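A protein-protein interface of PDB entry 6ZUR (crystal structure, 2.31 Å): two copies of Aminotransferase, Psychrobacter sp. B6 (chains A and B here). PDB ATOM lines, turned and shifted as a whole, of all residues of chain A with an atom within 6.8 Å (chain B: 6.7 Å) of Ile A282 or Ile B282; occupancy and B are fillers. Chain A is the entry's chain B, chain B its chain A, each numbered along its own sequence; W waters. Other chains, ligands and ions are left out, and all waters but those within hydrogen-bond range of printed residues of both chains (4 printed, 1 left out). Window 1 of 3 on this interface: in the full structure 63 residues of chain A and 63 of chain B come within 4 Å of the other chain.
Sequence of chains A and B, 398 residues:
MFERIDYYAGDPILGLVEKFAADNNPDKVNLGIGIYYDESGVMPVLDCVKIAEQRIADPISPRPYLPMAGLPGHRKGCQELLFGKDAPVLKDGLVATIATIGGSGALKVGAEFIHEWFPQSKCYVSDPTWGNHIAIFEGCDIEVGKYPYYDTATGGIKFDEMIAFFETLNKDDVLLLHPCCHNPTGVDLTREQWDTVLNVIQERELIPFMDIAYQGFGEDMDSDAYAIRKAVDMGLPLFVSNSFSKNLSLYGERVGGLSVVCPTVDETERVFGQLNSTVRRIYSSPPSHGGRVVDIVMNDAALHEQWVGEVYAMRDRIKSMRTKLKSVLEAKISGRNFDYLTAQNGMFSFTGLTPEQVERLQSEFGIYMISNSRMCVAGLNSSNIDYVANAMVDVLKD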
ATOM      1  N   ILE A 101     -23.706  -5.267   9.320  1.00  0.00           N
ATOM      2  CA  ILE A 101     -22.916  -4.022   9.497  1.00  0.00           C
ATOM      3  C   ILE A 101     -22.582  -3.499   8.123  1.00  0.00           C
ATOM      4  O   ILE A 101     -21.466  -3.674   7.635  1.00  0.00           O
ATOM      5  CB  ILE A 101     -21.569  -4.266  10.231  1.00  0.00           C
ATOM      6  CG1 ILE A 101     -21.670  -5.307  11.344  1.00  0.00           C
ATOM      7  CG2 ILE A 101     -21.060  -2.964  10.811  1.00  0.00           C
ATOM      8  CD1 ILE A 101     -22.683  -4.986  12.406  1.00  0.00           C
ATOM      9  N   SER A 104     -20.618  -4.248   3.599  1.00  0.00           N
ATOM     10  CA  SER A 104     -19.318  -4.856   3.940  1.00  0.00           C
ATOM     11  C   SER A 104     -19.455  -6.004   4.881  1.00  0.00           C
ATOM     12  O   SER A 104     -18.898  -7.078   4.636  1.00  0.00           O
ATOM     13  CB  SER A 104     -18.372  -3.834   4.540  1.00  0.00           C
ATOM     14  OG  SER A 104     -18.079  -2.809   3.571  1.00  0.00           O
ATOM     15  N   GLY A 105     -20.233  -5.771   5.931  1.00  0.00           N
ATOM     16  CA  GLY A 105     -20.568  -6.819   6.895  1.00  0.00           C
ATOM     17  C   GLY A 105     -21.247  -8.033   6.289  1.00  0.00           C
ATOM     18  O   GLY A 105     -20.943  -9.141   6.691  1.00  0.00           O
ATOM     19  N   ALA A 106     -22.170  -7.823   5.343  1.00  0.00           N
ATOM     20  CA  ALA A 106     -22.872  -8.903   4.655  1.00  0.00           C
ATOM     21  C   ALA A 106     -21.931  -9.717   3.755  1.00  0.00           C
ATOM     22  O   ALA A 106     -21.940 -10.960   3.737  1.00  0.00           O
ATOM     23  CB  ALA A 106     -24.008  -8.339   3.824  1.00  0.00           C
ATOM     24  N   LEU A 107     -21.084  -9.011   3.023  1.00  0.00           N
ATOM     25  CA  LEU A 107     -20.030  -9.673   2.334  1.00  0.00           C
ATOM     26  C   LEU A 107     -19.183 -10.508   3.258  1.00  0.00           C
ATOM     27  O   LEU A 107     -18.892 -11.685   2.918  1.00  0.00           O
ATOM     28  CB  LEU A 107     -19.122  -8.698   1.589  1.00  0.00           C
ATOM     29  CG  LEU A 107     -19.801  -8.045   0.413  1.00  0.00           C
ATOM     30  CD1 LEU A 107     -19.141  -6.730   0.086  1.00  0.00           C
ATOM     31  CD2 LEU A 107     -19.867  -8.970  -0.788  1.00  0.00           C
ATOM     32  N   LYS A 108     -18.810  -9.967   4.431  1.00  0.00           N
ATOM     33  CA  LYS A 108     -17.979 -10.750   5.346  1.00  0.00           C
ATOM     34  C   LYS A 108     -18.640 -12.055   5.861  1.00  0.00           C
ATOM     35  O   LYS A 108     -17.994 -13.102   5.940  1.00  0.00           O
ATOM     36  CB  LYS A 108     -17.576  -9.928   6.533  1.00  0.00           C
ATOM     37  CG  LYS A 108     -16.802 -10.719   7.613  1.00  0.00           C
ATOM     38  CD  LYS A 108     -15.488 -11.277   7.050  1.00  0.00           C
ATOM     39  CE  LYS A 108     -14.632 -11.874   8.169  1.00  0.00           C
ATOM     40  NZ  LYS A 108     -13.310 -12.323   7.643  1.00  0.00           N
ATOM     41  N   VAL A 109     -19.891 -11.947   6.301  1.00  0.00           N
ATOM     42  CA  VAL A 109     -20.622 -13.077   6.782  1.00  0.00           C
ATOM     43  C   VAL A 109     -20.835 -14.111   5.687  1.00  0.00           C
ATOM     44  O   VAL A 109     -20.704 -15.264   5.922  1.00  0.00           O
ATOM     45  CB  VAL A 109     -21.967 -12.647   7.453  1.00  0.00           C
ATOM     46  CG1 VAL A 109     -22.855 -13.863   7.855  1.00  0.00           C
ATOM     47  CG2 VAL A 109     -21.679 -11.885   8.742  1.00  0.00           C
ATOM     48  N   GLU A 112     -17.595 -15.806   4.942  1.00  0.00           N
ATOM     49  CA  GLU A 112     -17.196 -16.765   6.050  1.00  0.00           C
ATOM     50  C   GLU A 112     -18.021 -18.020   5.938  1.00  0.00           C
ATOM     51  O   GLU A 112     -17.538 -19.123   6.169  1.00  0.00           O
ATOM     52  CB  GLU A 112     -17.335 -16.213   7.461  1.00  0.00           C
ATOM     53  CG  GLU A 112     -16.286 -15.195   7.842  1.00  0.00           C
ATOM     54  CD  GLU A 112     -14.851 -15.717   8.044  1.00  0.00           C
ATOM     55  OE1 GLU A 112     -14.534 -16.837   7.635  1.00  0.00           O
ATOM     56  OE2 GLU A 112     -14.052 -14.995   8.660  1.00  0.00           O
ATOM     57  N   ASN A 132     -12.327  -3.399  -1.838  1.00  0.00           N
ATOM     58  CA  ASN A 132     -12.759  -4.168  -0.648  1.00  0.00           C
ATOM     59  C   ASN A 132     -13.347  -5.614  -0.857  1.00  0.00           C
ATOM     60  O   ASN A 132     -13.274  -6.426  -0.008  1.00  0.00           O
ATOM     61  CB  ASN A 132     -13.744  -3.377   0.189  1.00  0.00           C
ATOM     62  CG  ASN A 132     -13.635  -3.686   1.689  1.00  0.00           C
ATOM     63  OD1 ASN A 132     -12.570  -4.049   2.182  1.00  0.00           O
ATOM     64  ND2 ASN A 132     -14.725  -3.526   2.417  1.00  0.00           N
ATOM     65  N   ALA A 135     -10.438  -8.053  -0.514  1.00  0.00           N
ATOM     66  CA  ALA A 135      -9.924  -8.128   0.817  1.00  0.00           C
ATOM     67  C   ALA A 135     -10.847  -8.874   1.717  1.00  0.00           C
ATOM     68  O   ALA A 135     -10.390  -9.557   2.622  1.00  0.00           O
ATOM     69  CB  ALA A 135      -9.714  -6.746   1.391  1.00  0.00           C
ATOM     70  N   ILE A 136     -12.137  -8.673   1.542  1.00  0.00           N
ATOM     71  CA  ILE A 136     -13.092  -9.348   2.400  1.00  0.00           C
ATOM     72  C   ILE A 136     -13.003 -10.889   2.224  1.00  0.00           C
ATOM     73  O   ILE A 136     -12.879 -11.618   3.226  1.00  0.00           O
ATOM     74  CB  ILE A 136     -14.525  -8.837   2.170  1.00  0.00           C
ATOM     75  CG1 ILE A 136     -14.641  -7.447   2.730  1.00  0.00           C
ATOM     76  CG2 ILE A 136     -15.568  -9.722   2.867  1.00  0.00           C
ATOM     77  CD1 ILE A 136     -15.929  -6.728   2.442  1.00  0.00           C
ATOM     78  N   SER A 277     -24.931 -18.112  13.855  1.00  0.00           N
ATOM     79  CA  SER A 277     -23.703 -18.638  14.489  1.00  0.00           C
ATOM     80  C   SER A 277     -22.486 -17.919  13.976  1.00  0.00           C
ATOM     81  O   SER A 277     -21.514 -17.740  14.696  1.00  0.00           O
ATOM     82  CB  SER A 277     -23.521 -20.145  14.196  1.00  0.00           C
ATOM     83  OG  SER A 277     -22.340 -20.665  14.796  1.00  0.00           O
ATOM     84  N   THR A 278     -22.521 -17.526  12.707  1.00  0.00           N
ATOM     85  CA  THR A 278     -21.389 -16.785  12.135  1.00  0.00           C
ATOM     86  C   THR A 278     -21.380 -15.365  12.707  1.00  0.00           C
ATOM     87  O   THR A 278     -20.316 -14.803  13.072  1.00  0.00           O
ATOM     88  CB  THR A 278     -21.471 -16.762  10.602  1.00  0.00           C
ATOM     89  OG1 THR A 278     -21.555 -18.112  10.150  1.00  0.00           O
ATOM     90  CG2 THR A 278     -20.291 -16.055   9.968  1.00  0.00           C
ATOM     91  N   VAL A 279     -22.557 -14.779  12.825  1.00  0.00           N
ATOM     92  CA  VAL A 279     -22.624 -13.456  13.472  1.00  0.00           C
ATOM     93  C   VAL A 279     -22.071 -13.501  14.898  1.00  0.00           C
ATOM     94  O   VAL A 279     -21.334 -12.603  15.341  1.00  0.00           O
ATOM     95  CB  VAL A 279     -24.047 -12.887  13.404  1.00  0.00           C
ATOM     96  CG1 VAL A 279     -24.231 -11.762  14.362  1.00  0.00           C
ATOM     97  CG2 VAL A 279     -24.315 -12.489  11.955  1.00  0.00           C
ATOM     98  N   ARG A 280     -22.433 -14.545  15.609  1.00  0.00           N
ATOM     99  CA  ARG A 280     -22.015 -14.671  17.015  1.00  0.00           C
ATOM    100  C   ARG A 280     -20.515 -14.628  17.210  1.00  0.00           C
ATOM    101  O   ARG A 280     -19.990 -13.934  18.066  1.00  0.00           O
ATOM    102  CB  ARG A 280     -22.531 -15.979  17.588  1.00  0.00           C
ATOM    103  CG  ARG A 280     -22.290 -16.135  19.076  1.00  0.00           C
ATOM    104  CD  ARG A 280     -23.117 -17.289  19.627  1.00  0.00           C
ATOM    105  NE  ARG A 280     -22.929 -17.515  21.065  1.00  0.00           N
ATOM    106  CZ  ARG A 280     -21.861 -18.128  21.611  1.00  0.00           C
ATOM    107  NH1 ARG A 280     -20.837 -18.508  20.846  1.00  0.00           N
ATOM    108  NH2 ARG A 280     -21.802 -18.309  22.917  1.00  0.00           N
ATOM    109  N   ARG A 281     -19.824 -15.351  16.373  1.00  0.00           N
ATOM    110  CA  ARG A 281     -18.389 -15.367  16.417  1.00  0.00           C
ATOM    111  C   ARG A 281     -17.655 -14.156  15.861  1.00  0.00           C
ATOM    112  O   ARG A 281     -16.421 -14.047  16.068  1.00  0.00           O
ATOM    113  CB  ARG A 281     -17.836 -16.682  15.859  1.00  0.00           C
ATOM    114  CG  ARG A 281     -18.020 -16.947  14.405  1.00  0.00           C
ATOM    115  CD  ARG A 281     -17.754 -18.415  14.143  1.00  0.00           C
ATOM    116  NE  ARG A 281     -18.127 -18.807  12.783  1.00  0.00           N
ATOM    117  CZ  ARG A 281     -17.291 -18.801  11.730  1.00  0.00           C
ATOM    118  NH1 ARG A 281     -17.740 -19.148  10.519  1.00  0.00           N
ATOM    119  NH2 ARG A 281     -16.012 -18.399  11.880  1.00  0.00           N
ATOM    120  N   ILE A 282     -18.356 -13.224  15.218  1.00  0.00           N
ATOM    121  CA  ILE A 282     -17.703 -12.001  14.741  1.00  0.00           C
ATOM    122  C   ILE A 282     -17.948 -10.783  15.650  1.00  0.00           C
ATOM    123  O   ILE A 282     -17.012 -10.195  16.198  1.00  0.00           O
ATOM    124  CB  ILE A 282     -18.075 -11.683  13.280  1.00  0.00           C
ATOM    125  CG1 ILE A 282     -17.585 -12.815  12.371  1.00  0.00           C
ATOM    126  CG2 ILE A 282     -17.423 -10.382  12.867  1.00  0.00           C
ATOM    127  CD1 ILE A 282     -18.205 -12.843  10.985  1.00  0.00           C
ATOM    128  N   TYR A 283     -19.199 -10.359  15.751  1.00  0.00           N
ATOM    129  CA  TYR A 283     -19.538  -9.142  16.512  1.00  0.00           C
ATOM    130  C   TYR A 283     -20.791  -9.244  17.360  1.00  0.00           C
ATOM    131  O   TYR A 283     -21.225  -8.235  17.951  1.00  0.00           O
ATOM    132  CB  TYR A 283     -19.706  -7.957  15.523  1.00  0.00           C
ATOM    133  CG  TYR A 283     -20.750  -8.211  14.471  1.00  0.00           C
ATOM    134  CD1 TYR A 283     -22.100  -7.955  14.701  1.00  0.00           C
ATOM    135  CD2 TYR A 283     -20.383  -8.719  13.230  1.00  0.00           C
ATOM    136  CE1 TYR A 283     -23.036  -8.200  13.703  1.00  0.00           C
ATOM    137  CE2 TYR A 283     -21.300  -8.936  12.255  1.00  0.00           C
ATOM    138  CZ  TYR A 283     -22.625  -8.665  12.486  1.00  0.00           C
ATOM    139  OH  TYR A 283     -23.494  -8.958  11.456  1.00  0.00           O
ATOM    140  N   SER A 284     -21.373 -10.442  17.444  1.00  0.00           N
ATOM    141  CA  SER A 284     -22.456 -10.774  18.393  1.00  0.00           C
ATOM    142  C   SER A 284     -23.839 -10.290  17.977  1.00  0.00           C
ATOM    143  O   SER A 284     -24.768 -11.134  17.791  1.00  0.00           O
ATOM    144  CB  SER A 284     -22.057 -10.456  19.812  1.00  0.00           C
ATOM    145  OG  SER A 284     -23.054 -10.819  20.683  1.00  0.00           O
ATOM    146  N   SER A 285     -23.989  -9.002  17.672  1.00  0.00           N
ATOM    147  CA  SER A 285     -25.204  -8.529  17.019  1.00  0.00           C
ATOM    148  C   SER A 285     -25.054  -7.122  16.468  1.00  0.00           C
ATOM    149  O   SER A 285     -24.141  -6.389  16.860  1.00  0.00           O
ATOM    150  CB  SER A 285     -26.397  -8.543  18.038  1.00  0.00           C
ATOM    151  OG  SER A 285     -26.104  -7.757  19.140  1.00  0.00           O
ATOM    152  N   ILE B 101     -17.037  -2.928  17.543  1.00  0.00           N
ATOM    153  CA  ILE B 101     -18.419  -3.300  17.603  1.00  0.00           C
ATOM    154  C   ILE B 101     -18.595  -4.016  18.941  1.00  0.00           C
ATOM    155  O   ILE B 101     -18.660  -5.264  19.006  1.00  0.00           O
ATOM    156  CB  ILE B 101     -18.842  -4.270  16.471  1.00  0.00           C
ATOM    157  CG1 ILE B 101     -18.222  -3.933  15.098  1.00  0.00           C
ATOM    158  CG2 ILE B 101     -20.355  -4.307  16.376  1.00  0.00           C
ATOM    159  CD1 ILE B 101     -18.633  -2.580  14.576  1.00  0.00           C
ATOM    160  N   SER B 104     -17.115  -7.743  22.021  1.00  0.00           N
ATOM    161  CA  SER B 104     -17.049  -8.863  21.104  1.00  0.00           C
ATOM    162  C   SER B 104     -16.231  -8.548  19.864  1.00  0.00           C
ATOM    163  O   SER B 104     -15.383  -9.327  19.469  1.00  0.00           O
ATOM    164  CB  SER B 104     -18.433  -9.216  20.620  1.00  0.00           C
ATOM    165  OG  SER B 104     -19.223  -9.468  21.733  1.00  0.00           O
ATOM    166  N   GLY B 105     -16.550  -7.409  19.246  1.00  0.00           N
ATOM    167  CA  GLY B 105     -15.872  -6.933  18.098  1.00  0.00           C
ATOM    168  C   GLY B 105     -14.423  -6.656  18.289  1.00  0.00           C
ATOM    169  O   GLY B 105     -13.631  -6.945  17.358  1.00  0.00           O
ATOM    170  N   ALA B 106     -14.057  -6.120  19.456  1.00  0.00           N
ATOM    171  CA  ALA B 106     -12.621  -5.971  19.832  1.00  0.00           C
ATOM    172  C   ALA B 106     -11.917  -7.329  20.007  1.00  0.00           C
ATOM    173  O   ALA B 106     -10.770  -7.541  19.536  1.00  0.00           O
ATOM    174  CB  ALA B 106     -12.470  -5.168  21.105  1.00  0.00           C
ATOM    175  N   LEU B 107     -12.573  -8.254  20.705  1.00  0.00           N
ATOM    176  CA  LEU B 107     -12.042  -9.609  20.767  1.00  0.00           C
ATOM    177  C   LEU B 107     -11.808 -10.179  19.366  1.00  0.00           C
ATOM    178  O   LEU B 107     -10.779 -10.814  19.130  1.00  0.00           O
ATOM    179  CB  LEU B 107     -12.967 -10.553  21.539  1.00  0.00           C
ATOM    180  CG  LEU B 107     -13.007 -10.305  23.017  1.00  0.00           C
ATOM    181  CD1 LEU B 107     -14.312 -10.789  23.651  1.00  0.00           C
ATOM    182  CD2 LEU B 107     -11.753 -10.857  23.683  1.00  0.00           C
ATOM    183  N   LYS B 108     -12.762  -9.977  18.455  1.00  0.00           N
ATOM    184  CA  LYS B 108     -12.603 -10.508  17.083  1.00  0.00           C
ATOM    185  C   LYS B 108     -11.416  -9.952  16.335  1.00  0.00           C
ATOM    186  O   LYS B 108     -10.658 -10.711  15.737  1.00  0.00           O
ATOM    187  CB  LYS B 108     -13.865 -10.284  16.272  1.00  0.00           C
ATOM    188  CG  LYS B 108     -13.809 -10.773  14.839  1.00  0.00           C
ATOM    189  CD  LYS B 108     -13.429 -12.232  14.709  1.00  0.00           C
ATOM    190  CE  LYS B 108     -13.507 -12.656  13.265  1.00  0.00           C
ATOM    191  NZ  LYS B 108     -13.295 -14.146  13.142  1.00  0.00           N
ATOM    192  N   VAL B 109     -11.281  -8.621  16.326  1.00  0.00           N
ATOM    193  CA  VAL B 109     -10.199  -7.960  15.632  1.00  0.00           C
ATOM    194  C   VAL B 109      -8.863  -8.335  16.270  1.00  0.00           C
ATOM    195  O   VAL B 109      -7.897  -8.583  15.575  1.00  0.00           O
ATOM    196  CB  VAL B 109     -10.371  -6.450  15.611  1.00  0.00           C
ATOM    197  CG1 VAL B 109      -9.162  -5.756  15.015  1.00  0.00           C
ATOM    198  CG2 VAL B 109     -11.571  -6.089  14.760  1.00  0.00           C
ATOM    199  N   GLU B 112      -8.070 -11.936  15.298  1.00  0.00           N
ATOM    200  CA  GLU B 112      -7.701 -12.030  13.898  1.00  0.00           C
ATOM    201  C   GLU B 112      -6.277 -11.507  13.681  1.00  0.00           C
ATOM    202  O   GLU B 112      -5.503 -12.076  12.885  1.00  0.00           O
ATOM    203  CB  GLU B 112      -8.681 -11.179  13.115  1.00  0.00           C
ATOM    204  CG  GLU B 112      -9.227 -11.643  11.830  1.00  0.00           C
ATOM    205  CD  GLU B 112      -9.498 -13.141  11.692  1.00  0.00           C
ATOM    206  OE1 GLU B 112     -10.701 -13.531  11.755  1.00  0.00           O
ATOM    207  OE2 GLU B 112      -8.528 -13.888  11.413  1.00  0.00           O
ATOM    208  N   ASN B 132     -18.780 -17.095  24.787  1.00  0.00           N
ATOM    209  CA  ASN B 132     -18.415 -16.360  23.554  1.00  0.00           C
ATOM    210  C   ASN B 132     -16.890 -16.161  23.284  1.00  0.00           C
ATOM    211  O   ASN B 132     -16.485 -15.966  22.155  1.00  0.00           O
ATOM    212  CB  ASN B 132     -19.156 -15.044  23.624  1.00  0.00           C
ATOM    213  CG  ASN B 132     -18.905 -14.144  22.460  1.00  0.00           C
ATOM    214  OD1 ASN B 132     -18.125 -13.217  22.587  1.00  0.00           O
ATOM    215  ND2 ASN B 132     -19.598 -14.376  21.336  1.00  0.00           N
ATOM    216  N   ALA B 135     -15.652 -19.141  21.161  1.00  0.00           N
ATOM    217  CA  ALA B 135     -16.121 -19.047  19.776  1.00  0.00           C
ATOM    218  C   ALA B 135     -15.373 -18.036  18.939  1.00  0.00           C
ATOM    219  O   ALA B 135     -15.155 -18.269  17.792  1.00  0.00           O
ATOM    220  CB  ALA B 135     -17.585 -18.726  19.728  1.00  0.00           C
ATOM    221  N   ILE B 136     -15.040 -16.909  19.523  1.00  0.00           N
ATOM    222  CA  ILE B 136     -14.452 -15.818  18.780  1.00  0.00           C
ATOM    223  C   ILE B 136     -13.066 -16.164  18.301  1.00  0.00           C
ATOM    224  O   ILE B 136     -12.781 -16.017  17.075  1.00  0.00           O
ATOM    225  CB  ILE B 136     -14.446 -14.542  19.586  1.00  0.00           C
ATOM    226  CG1 ILE B 136     -15.854 -13.970  19.658  1.00  0.00           C
ATOM    227  CG2 ILE B 136     -13.554 -13.516  18.942  1.00  0.00           C
ATOM    228  CD1 ILE B 136     -16.033 -12.830  20.692  1.00  0.00           C
ATOM    229  N   SER B 277      -6.585  -2.298   8.822  1.00  0.00           N
ATOM    230  CA  SER B 277      -6.681  -3.214   7.727  1.00  0.00           C
ATOM    231  C   SER B 277      -7.560  -4.355   8.067  1.00  0.00           C
ATOM    232  O   SER B 277      -8.293  -4.822   7.241  1.00  0.00           O
ATOM    233  CB  SER B 277      -5.299  -3.808   7.313  1.00  0.00           C
ATOM    234  OG  SER B 277      -5.442  -4.662   6.162  1.00  0.00           O
ATOM    235  N   THR B 278      -7.444  -4.842   9.283  1.00  0.00           N
ATOM    236  CA  THR B 278      -8.338  -5.911   9.782  1.00  0.00           C
ATOM    237  C   THR B 278      -9.787  -5.458   9.856  1.00  0.00           C
ATOM    238  O   THR B 278     -10.684  -6.213   9.524  1.00  0.00           O
ATOM    239  CB  THR B 278      -7.867  -6.377  11.146  1.00  0.00           C
ATOM    240  OG1 THR B 278      -6.478  -6.685  11.051  1.00  0.00           O
ATOM    241  CG2 THR B 278      -8.636  -7.585  11.593  1.00  0.00           C
ATOM    242  N   VAL B 279     -10.005  -4.221  10.294  1.00  0.00           N
ATOM    243  CA  VAL B 279     -11.360  -3.678  10.297  1.00  0.00           C
ATOM    244  C   VAL B 279     -11.958  -3.572   8.894  1.00  0.00           C
ATOM    245  O   VAL B 279     -13.096  -3.928   8.659  1.00  0.00           O
ATOM    246  CB  VAL B 279     -11.420  -2.298  10.975  1.00  0.00           C
ATOM    247  CG1 VAL B 279     -12.731  -1.592  10.580  1.00  0.00           C
ATOM    248  CG2 VAL B 279     -11.276  -2.500  12.481  1.00  0.00           C
ATOM    249  N   ARG B 280     -11.134  -3.122   7.977  1.00  0.00           N
ATOM    250  CA  ARG B 280     -11.513  -2.953   6.578  1.00  0.00           C
ATOM    251  C   ARG B 280     -11.981  -4.278   6.019  1.00  0.00           C
ATOM    252  O   ARG B 280     -12.921  -4.322   5.276  1.00  0.00           O
ATOM    253  CB  ARG B 280     -10.321  -2.434   5.788  1.00  0.00           C
ATOM    254  CG  ARG B 280     -10.690  -2.123   4.351  1.00  0.00           C
ATOM    255  CD  ARG B 280      -9.516  -1.480   3.683  1.00  0.00           C
ATOM    256  NE  ARG B 280      -9.624  -1.236   2.248  1.00  0.00           N
ATOM    257  CZ  ARG B 280      -9.424  -2.156   1.312  1.00  0.00           C
ATOM    258  NH1 ARG B 280      -9.218  -3.434   1.656  1.00  0.00           N
ATOM    259  NH2 ARG B 280      -9.493  -1.821   0.033  1.00  0.00           N
ATOM    260  N   ARG B 281     -11.357  -5.363   6.467  1.00  0.00           N
ATOM    261  CA  ARG B 281     -11.710  -6.709   6.008  1.00  0.00           C
ATOM    262  C   ARG B 281     -12.961  -7.278   6.579  1.00  0.00           C
ATOM    263  O   ARG B 281     -13.467  -8.255   6.052  1.00  0.00           O
ATOM    264  CB  ARG B 281     -10.585  -7.691   6.392  1.00  0.00           C
ATOM    265  CG  ARG B 281      -9.640  -7.854   5.267  1.00  0.00           C
ATOM    266  CD  ARG B 281      -8.249  -7.889   5.727  1.00  0.00           C
ATOM    267  NE  ARG B 281      -7.919  -8.888   6.712  1.00  0.00           N
ATOM    268  CZ  ARG B 281      -6.795  -8.885   7.416  1.00  0.00           C
ATOM    269  NH1 ARG B 281      -5.900  -7.880   7.255  1.00  0.00           N
ATOM    270  NH2 ARG B 281      -6.568  -9.836   8.314  1.00  0.00           N
ATOM    271  N   ILE B 282     -13.405  -6.761   7.720  1.00  0.00           N
ATOM    272  CA  ILE B 282     -14.541  -7.400   8.394  1.00  0.00           C
ATOM    273  C   ILE B 282     -15.814  -6.616   8.160  1.00  0.00           C
ATOM    274  O   ILE B 282     -16.758  -7.173   7.674  1.00  0.00           O
ATOM    275  CB  ILE B 282     -14.282  -7.569   9.911  1.00  0.00           C
ATOM    276  CG1 ILE B 282     -13.137  -8.546  10.107  1.00  0.00           C
ATOM    277  CG2 ILE B 282     -15.518  -8.088  10.603  1.00  0.00           C
ATOM    278  CD1 ILE B 282     -12.511  -8.582  11.476  1.00  0.00           C
ATOM    279  N   TYR B 283     -15.837  -5.354   8.584  1.00  0.00           N
ATOM    280  CA  TYR B 283     -17.068  -4.551   8.504  1.00  0.00           C
ATOM    281  C   TYR B 283     -16.814  -3.107   8.087  1.00  0.00           C
ATOM    282  O   TYR B 283     -17.758  -2.324   8.118  1.00  0.00           O
ATOM    283  CB  TYR B 283     -17.832  -4.605   9.879  1.00  0.00           C
ATOM    284  CG  TYR B 283     -16.975  -4.105  11.004  1.00  0.00           C
ATOM    285  CD1 TYR B 283     -16.802  -2.729  11.268  1.00  0.00           C
ATOM    286  CD2 TYR B 283     -16.252  -4.988  11.756  1.00  0.00           C
ATOM    287  CE1 TYR B 283     -16.014  -2.322  12.288  1.00  0.00           C
ATOM    288  CE2 TYR B 283     -15.420  -4.562  12.774  1.00  0.00           C
ATOM    289  CZ  TYR B 283     -15.315  -3.232  13.026  1.00  0.00           C
ATOM    290  OH  TYR B 283     -14.490  -2.844  14.031  1.00  0.00           O
ATOM    291  N   SER B 284     -15.568  -2.771   7.735  1.00  0.00           N
ATOM    292  CA  SER B 284     -15.193  -1.536   7.074  1.00  0.00           C
ATOM    293  C   SER B 284     -15.067  -0.352   8.032  1.00  0.00           C
ATOM    294  O   SER B 284     -14.029   0.306   8.065  1.00  0.00           O
ATOM    295  CB  SER B 284     -16.119  -1.243   5.872  1.00  0.00           C
ATOM    296  OG  SER B 284     -15.761  -0.022   5.257  1.00  0.00           O
ATOM    297  N   SER B 285     -16.129  -0.021   8.783  1.00  0.00           N
ATOM    298  CA  SER B 285     -16.018   0.960   9.852  1.00  0.00           C
ATOM    299  C   SER B 285     -17.148   0.784  10.927  1.00  0.00           C
ATOM    300  O   SER B 285     -18.205   0.243  10.649  1.00  0.00           O
ATOM    301  CB  SER B 285     -16.021   2.380   9.253  1.00  0.00           C
ATOM    302  OG  SER B 285     -17.253   2.643   8.575  1.00  0.00           O
HETATM  303  O   HOH W   1     -14.416 -15.692  15.319  1.00  0.00           O
HETATM  304  O   HOH W   2     -11.671 -11.767   9.877  1.00  0.00           O
HETATM  305  O   HOH W   3     -12.497 -11.146   5.569  1.00  0.00           O
HETATM  306  O   HOH W   4     -15.066 -14.436  10.943  1.00  0.00           O
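The side-chain amide nitrogen (ND2) of Asn B132 is in hydrogen-bond range of the backbone carbonyl oxygen (O) of Arg A280 (3.3 Å).
O of Arg B280 sits close to OD1 of Asn A132 (3.1 Å).
The backbone NH (N) of Ser B284 sits at hydrogen-bond distance from the backbone carbonyl oxygen (O) of Val B279 (2.9 Å).
NZ of Lys A108 is in salt-bridge range of OE2 of Glu A112, at 3.0 Å.
Among the printed residues, pairs that only touch across the chains: Lys A108 with Ile B282 (3.1 Å), Ile A282 with Lys B108 (3.1 Å), Ala A135 with Arg B281 (3.2 Å), Ala A135 with Arg B280 (3.4 Å), Ser A104 with Ser B284 (3.4 Å), Arg A280 with Ala B135 (3.4 Å), Ser A284 with Ser B104 (3.6 Å), Ile A136 with Arg B281 (3.6 Å), Arg A281 with Ile B136 (3.6 Å), Arg A281 with Ala B135 (3.7 Å), Ser A104 with Ile B282 (3.7 Å), Ile A101 with Tyr B283 (3.7 Å), Ile A282 with Ile B282 (3.7 Å), Arg A281 with Lys B108 (3.8 Å), Ile A282 with Ser B104 (3.8 Å), Lys A108 with Arg B281 (3.8 Å), Tyr A283 with Ile B101 (3.8 Å), Gly A105 with Ile B282 (3.9 Å), Ser A104 with Tyr B283 (3.9 Å), Ile A282 with Gly B105 (3.9 Å) and Tyr A283 with Ser B104 (3.99 Å).
Of the printed residues of chain B, Ile A282 touches Ser B104 (3.8 Å), Gly B105 (3.9 Å), Lys B108 (3.1 Å) and Ile B282 (3.7 Å).
Ile B282 touches four residues of chain A.
Of the printed residues of chain A, Gly B105 touches Ile A282.
Of the printed residues of chain B, Arg A281 touches Lys B108, Ala B135 and Ile B136.
The nearest residue of chain B that does not touch Ile A282 is Ile B136 (5.2 Å).
The nearest residue of chain A that does not touch Ile B282 is Ile A136 (5.2 Å).
Of the 20 printed residues of chain B, 12 touch a printed residue of chain A.
Of the 20 printed residues of chain A, 12 touch a printed residue of chain B.
Along chain A the printed residues that touch a printed residue of chain B span positions 101 to 284.
Among the printed residues, 23 pairs touch across the chains.
Among the printed residues, no Asp or Glu carboxylate lies within 4 Å of a Lys or Arg side-chain nitrogen of the other chain.
Ser A104 touches Ile B282, and with the chains exchanged Ile A282 touches Ser B104.
Gly A105 touches Ile B282, and with the chains exchanged Ile A282 touches Gly B105.
Water W1 lies within hydrogen-bond range of O of Ile B136 (2.4 Å), O of Arg A281 (2.7 Å) and NZ of Lys B108 (2.9 Å).
Water W4 bridges the side-chain carboxylate (OE2) of Glu A112 (2.6 Å) and the side-chain amino group (NZ) of Lys B108 (2.8 Å).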
